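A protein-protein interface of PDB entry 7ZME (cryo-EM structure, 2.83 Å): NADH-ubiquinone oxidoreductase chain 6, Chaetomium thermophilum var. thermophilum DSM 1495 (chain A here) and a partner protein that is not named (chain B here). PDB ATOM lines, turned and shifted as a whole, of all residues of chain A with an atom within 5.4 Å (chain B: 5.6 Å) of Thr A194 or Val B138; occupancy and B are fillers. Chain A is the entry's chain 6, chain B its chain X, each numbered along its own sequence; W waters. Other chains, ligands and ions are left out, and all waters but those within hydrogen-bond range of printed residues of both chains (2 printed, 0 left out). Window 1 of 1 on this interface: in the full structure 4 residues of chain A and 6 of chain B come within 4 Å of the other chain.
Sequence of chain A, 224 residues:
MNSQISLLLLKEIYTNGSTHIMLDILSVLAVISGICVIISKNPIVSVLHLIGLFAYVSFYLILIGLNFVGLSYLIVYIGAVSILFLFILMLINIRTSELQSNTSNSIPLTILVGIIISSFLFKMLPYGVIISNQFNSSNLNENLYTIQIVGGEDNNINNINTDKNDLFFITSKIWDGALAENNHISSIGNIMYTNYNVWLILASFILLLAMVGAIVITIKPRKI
Met A192 touches none of the printed residues of chain B.
Of the printed residues of chain B, Asn A195 touches Val B138 (3.4 Å) and Arg B141 (3.8 Å).
Printed residues of chain A within 4 Å of Met B135: Thr A194 (3.6 Å).
Of chain A, only Thr A194 (3.6 Å) and Asn A195 (3.4 Å) come within 4 Å of Val B138.
Ala B140 touches none of the printed residues of chain A.
The nearest residue of chain B that does not touch Thr A194 is Gln B142 (4.6 Å).
The nearest printed residue of chain A that does not touch Met B135 is Asn A195 (4.4 Å).
Water W2 lies within hydrogen-bond range of O of Thr A194 (2.4 Å), NE2 of Gln B142 (2.6 Å) and ND2 of Asn A197 (3.2 Å).
Water W1 lies within hydrogen-bond range of the side-chain amide oxygen of Asn A197 and the side-chain amide nitrogen of Gln B142.
OD1 of Asn A197 lies close to OE1 of Gln B142 (3.2 Å).
The backbone carbonyl oxygen of Asn A190 is in hydrogen-bond range of the side-chain hydroxyl of Thr A194 (3.4 Å).
The side-chain hydroxyl (OG1) of Thr A194 is in hydrogen-bond range of the side-chain amide oxygen (OD1) of Asn A195 (2.8 Å).
The backbone carbonyl oxygen (O) of Thr A194 is in hydrogen-bond range of the side-chain amide nitrogen (ND2) of Asn A197 (3.2 Å).
Of the 8 printed residues of chain A, 3 touch a printed residue of chain B.
Hydrophobic or aromatic side chains of chain B within 4 Å of the printed part of chain A: Met B135 and Val B138.
Along chain B the printed residues that touch a printed residue of chain A span positions 135 to 142.
Thr A194 touches Met B135.
CG1 of Val B138 touches C of Thr A194, at 3.6 Å.
ND2 of Asn A195 touches CG2 of Val B138 (3.4 Å).
Arg B141 touches Asn A195 (NH1 to ND2, 3.8 Å).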
ATOM      1  N   ASN A 190       2.345  -2.500  30.254  1.00  0.00           N
ATOM      2  CA  ASN A 190       2.201  -3.647  29.363  1.00  0.00           C
ATOM      3  C   ASN A 190       3.522  -4.061  28.728  1.00  0.00           C
ATOM      4  O   ASN A 190       3.676  -5.226  28.350  1.00  0.00           O
ATOM      5  CB  ASN A 190       1.185  -3.333  28.266  1.00  0.00           C
ATOM      6  CG  ASN A 190      -0.249  -3.355  28.763  1.00  0.00           C
ATOM      7  OD1 ASN A 190      -1.162  -2.921  28.065  1.00  0.00           O
ATOM      8  ND2 ASN A 190      -0.452  -3.859  29.970  1.00  0.00           N
ATOM      9  N   ILE A 191       4.474  -3.138  28.607  1.00  0.00           N
ATOM     10  CA  ILE A 191       5.725  -3.400  27.901  1.00  0.00           C
ATOM     11  C   ILE A 191       6.961  -3.111  28.733  1.00  0.00           C
ATOM     12  O   ILE A 191       8.058  -3.578  28.384  1.00  0.00           O
ATOM     13  CB  ILE A 191       5.769  -2.584  26.595  1.00  0.00           C
ATOM     14  CG1 ILE A 191       5.660  -1.100  26.931  1.00  0.00           C
ATOM     15  CG2 ILE A 191       4.653  -3.002  25.665  1.00  0.00           C
ATOM     16  CD1 ILE A 191       5.963  -0.202  25.796  1.00  0.00           C
ATOM     17  N   MET A 192       6.851  -2.356  29.823  1.00  0.00           N
ATOM     18  CA  MET A 192       8.013  -1.920  30.585  1.00  0.00           C
ATOM     19  C   MET A 192       8.704  -3.068  31.310  1.00  0.00           C
ATOM     20  O   MET A 192       9.873  -2.941  31.687  1.00  0.00           O
ATOM     21  CB  MET A 192       7.563  -0.830  31.561  1.00  0.00           C
ATOM     22  CG  MET A 192       8.506  -0.468  32.675  1.00  0.00           C
ATOM     23  SD  MET A 192       7.663   0.618  33.823  1.00  0.00           S
ATOM     24  CE  MET A 192       9.053   1.358  34.651  1.00  0.00           C
ATOM     25  N   TYR A 193       8.017  -4.191  31.498  1.00  0.00           N
ATOM     26  CA  TYR A 193       8.600  -5.283  32.316  1.00  0.00           C
ATOM     27  C   TYR A 193       8.747  -6.547  31.474  1.00  0.00           C
ATOM     28  O   TYR A 193       9.088  -7.596  32.024  1.00  0.00           O
ATOM     29  CB  TYR A 193       7.737  -5.527  33.554  1.00  0.00           C
ATOM     30  CG  TYR A 193       7.421  -4.300  34.369  1.00  0.00           C
ATOM     31  CD1 TYR A 193       8.266  -3.874  35.375  1.00  0.00           C
ATOM     32  CD2 TYR A 193       6.272  -3.568  34.130  1.00  0.00           C
ATOM     33  CE1 TYR A 193       7.984  -2.747  36.125  1.00  0.00           C
ATOM     34  CE2 TYR A 193       5.977  -2.434  34.863  1.00  0.00           C
ATOM     35  CZ  TYR A 193       6.833  -2.027  35.868  1.00  0.00           C
ATOM     36  OH  TYR A 193       6.537  -0.916  36.598  1.00  0.00           O
ATOM     37  N   THR A 194       8.479  -6.449  30.176  1.00  0.00           N
ATOM     38  CA  THR A 194       8.674  -7.604  29.272  1.00  0.00           C
ATOM     39  C   THR A 194       9.412  -7.148  28.026  1.00  0.00           C
ATOM     40  O   THR A 194      10.608  -7.401  27.961  1.00  0.00           O
ATOM     41  CB  THR A 194       7.334  -8.229  28.867  1.00  0.00           C
ATOM     42  OG1 THR A 194       6.468  -7.228  28.334  1.00  0.00           O
ATOM     43  CG2 THR A 194       6.644  -8.939  30.010  1.00  0.00           C
ATOM     44  N   ASN A 195       8.751  -6.414  27.139  1.00  0.00           N
ATOM     45  CA  ASN A 195       9.321  -6.033  25.820  1.00  0.00           C
ATOM     46  C   ASN A 195      10.582  -5.187  25.988  1.00  0.00           C
ATOM     47  O   ASN A 195      11.499  -5.342  25.177  1.00  0.00           O
ATOM     48  CB  ASN A 195       8.264  -5.304  24.993  1.00  0.00           C
ATOM     49  CG  ASN A 195       6.981  -6.081  24.794  1.00  0.00           C
ATOM     50  OD1 ASN A 195       6.207  -6.274  25.726  1.00  0.00           O
ATOM     51  ND2 ASN A 195       6.730  -6.508  23.570  1.00  0.00           N
ATOM     52  N   TYR A 196      10.612  -4.313  26.991  1.00  0.00           N
ATOM     53  CA  TYR A 196      11.756  -3.390  27.192  1.00  0.00           C
ATOM     54  C   TYR A 196      12.384  -3.599  28.577  1.00  0.00           C
ATOM     55  O   TYR A 196      12.895  -2.626  29.130  1.00  0.00           O
ATOM     56  CB  TYR A 196      11.313  -1.963  26.860  1.00  0.00           C
ATOM     57  CG  TYR A 196      10.767  -1.822  25.462  1.00  0.00           C
ATOM     58  CD1 TYR A 196      11.608  -1.600  24.387  1.00  0.00           C
ATOM     59  CD2 TYR A 196       9.414  -1.963  25.204  1.00  0.00           C
ATOM     60  CE1 TYR A 196      11.120  -1.491  23.097  1.00  0.00           C
ATOM     61  CE2 TYR A 196       8.911  -1.879  23.918  1.00  0.00           C
ATOM     62  CZ  TYR A 196       9.766  -1.634  22.859  1.00  0.00           C
ATOM     63  OH  TYR A 196       9.274  -1.534  21.591  1.00  0.00           O
ATOM     64  N   ASN A 197      12.394  -4.827  29.096  1.00  0.00           N
ATOM     65  CA  ASN A 197      12.906  -5.118  30.464  1.00  0.00           C
ATOM     66  C   ASN A 197      14.398  -4.773  30.611  1.00  0.00           C
ATOM     67  O   ASN A 197      14.829  -4.584  31.748  1.00  0.00           O
ATOM     68  CB  ASN A 197      12.534  -6.534  30.928  1.00  0.00           C
ATOM     69  CG  ASN A 197      13.162  -7.667  30.143  1.00  0.00           C
ATOM     70  OD1 ASN A 197      14.247  -7.531  29.586  1.00  0.00           O
ATOM     71  ND2 ASN A 197      12.497  -8.809  30.125  1.00  0.00           N
ATOM     72  N   ALA B 134       1.357 -13.942  22.852  1.00  0.00           N
ATOM     73  CA  ALA B 134       2.186 -12.761  22.641  1.00  0.00           C
ATOM     74  C   ALA B 134       3.289 -12.651  23.684  1.00  0.00           C
ATOM     75  O   ALA B 134       4.385 -12.178  23.369  1.00  0.00           O
ATOM     76  CB  ALA B 134       1.321 -11.503  22.640  1.00  0.00           C
ATOM     77  N   MET B 135       3.016 -13.122  24.902  1.00  0.00           N
ATOM     78  CA  MET B 135       4.032 -13.071  25.979  1.00  0.00           C
ATOM     79  C   MET B 135       5.056 -14.159  25.698  1.00  0.00           C
ATOM     80  O   MET B 135       6.205 -14.005  26.127  1.00  0.00           O
ATOM     81  CB  MET B 135       3.379 -13.333  27.333  1.00  0.00           C
ATOM     82  CG  MET B 135       2.887 -12.077  28.012  1.00  0.00           C
ATOM     83  SD  MET B 135       4.203 -10.852  28.188  1.00  0.00           S
ATOM     84  CE  MET B 135       3.689  -9.623  26.988  1.00  0.00           C
ATOM     85  N   GLN B 136       4.634 -15.204  24.987  1.00  0.00           N
ATOM     86  CA  GLN B 136       5.526 -16.313  24.589  1.00  0.00           C
ATOM     87  C   GLN B 136       6.518 -15.766  23.581  1.00  0.00           C
ATOM     88  O   GLN B 136       7.680 -16.178  23.617  1.00  0.00           O
ATOM     89  CB  GLN B 136       4.702 -17.435  23.958  1.00  0.00           C
ATOM     90  CG  GLN B 136       3.896 -18.253  24.954  1.00  0.00           C
ATOM     91  CD  GLN B 136       3.099 -19.321  24.253  1.00  0.00           C
ATOM     92  OE1 GLN B 136       3.604 -20.026  23.385  1.00  0.00           O
ATOM     93  NE2 GLN B 136       1.839 -19.455  24.629  1.00  0.00           N
ATOM     94  N   GLY B 137       6.040 -14.900  22.688  1.00  0.00           N
ATOM     95  CA  GLY B 137       6.882 -14.259  21.666  1.00  0.00           C
ATOM     96  C   GLY B 137       7.867 -13.300  22.275  1.00  0.00           C
ATOM     97  O   GLY B 137       9.028 -13.344  21.878  1.00  0.00           O
ATOM     98  N   VAL B 138       7.416 -12.467  23.204  1.00  0.00           N
ATOM     99  CA  VAL B 138       8.336 -11.534  23.912  1.00  0.00           C
ATOM    100  C   VAL B 138       9.426 -12.365  24.596  1.00  0.00           C
ATOM    101  O   VAL B 138      10.573 -11.918  24.599  1.00  0.00           O
ATOM    102  CB  VAL B 138       7.566 -10.638  24.906  1.00  0.00           C
ATOM    103  CG1 VAL B 138       8.485  -9.712  25.679  1.00  0.00           C
ATOM    104  CG2 VAL B 138       6.465  -9.848  24.224  1.00  0.00           C
ATOM    105  N   ALA B 139       9.101 -13.566  25.069  1.00  0.00           N
ATOM    106  CA  ALA B 139      10.064 -14.403  25.811  1.00  0.00           C
ATOM    107  C   ALA B 139      11.042 -15.038  24.827  1.00  0.00           C
ATOM    108  O   ALA B 139      12.242 -15.015  25.121  1.00  0.00           O
ATOM    109  CB  ALA B 139       9.307 -15.457  26.563  1.00  0.00           C
ATOM    110  N   ALA B 140      10.558 -15.599  23.719  1.00  0.00           N
ATOM    111  CA  ALA B 140      11.433 -16.121  22.648  1.00  0.00           C
ATOM    112  C   ALA B 140      12.392 -15.015  22.196  1.00  0.00           C
ATOM    113  O   ALA B 140      13.588 -15.284  22.106  1.00  0.00           O
ATOM    114  CB  ALA B 140      10.551 -16.565  21.517  1.00  0.00           C
ATOM    115  N   ARG B 141      11.879 -13.820  21.939  1.00  0.00           N
ATOM    116  CA  ARG B 141      12.685 -12.670  21.459  1.00  0.00           C
ATOM    117  C   ARG B 141      13.745 -12.292  22.494  1.00  0.00           C
ATOM    118  O   ARG B 141      14.857 -11.946  22.091  1.00  0.00           O
ATOM    119  CB  ARG B 141      11.790 -11.556  20.913  1.00  0.00           C
ATOM    120  CG  ARG B 141      10.945 -12.000  19.728  1.00  0.00           C
ATOM    121  CD  ARG B 141      10.138 -10.906  19.066  1.00  0.00           C
ATOM    122  NE  ARG B 141       9.409 -10.035  19.975  1.00  0.00           N
ATOM    123  CZ  ARG B 141       8.106 -10.102  20.209  1.00  0.00           C
ATOM    124  NH1 ARG B 141       7.541  -9.253  21.046  1.00  0.00           N
ATOM    125  NH2 ARG B 141       7.367 -11.010  19.598  1.00  0.00           N
ATOM    126  N   GLN B 142      13.392 -12.316  23.775  1.00  0.00           N
ATOM    127  CA  GLN B 142      14.334 -11.967  24.871  1.00  0.00           C
ATOM    128  C   GLN B 142      15.462 -12.981  25.033  1.00  0.00           C
ATOM    129  O   GLN B 142      16.593 -12.551  25.276  1.00  0.00           O
ATOM    130  CB  GLN B 142      13.569 -11.836  26.184  1.00  0.00           C
ATOM    131  CG  GLN B 142      14.441 -11.790  27.432  1.00  0.00           C
ATOM    132  CD  GLN B 142      14.963 -10.418  27.783  1.00  0.00           C
ATOM    133  OE1 GLN B 142      15.703 -10.244  28.744  1.00  0.00           O
ATOM    134  NE2 GLN B 142      14.579  -9.424  27.003  1.00  0.00           N
ATOM    135  N   SER B 143      15.180 -14.271  24.880  1.00  0.00           N
ATOM    136  CA  SER B 143      16.193 -15.297  25.218  1.00  0.00           C
ATOM    137  C   SER B 143      16.870 -15.975  24.029  1.00  0.00           C
ATOM    138  O   SER B 143      17.791 -16.747  24.288  1.00  0.00           O
ATOM    139  CB  SER B 143      15.588 -16.303  26.143  1.00  0.00           C
ATOM    140  OG  SER B 143      14.267 -16.626  25.755  1.00  0.00           O
HETATM  141  O   HOH W   1      14.429  -6.354  26.857  1.00  0.00           O
HETATM  142  O   HOH W   2      11.946  -9.180  26.972  1.00  0.00           O
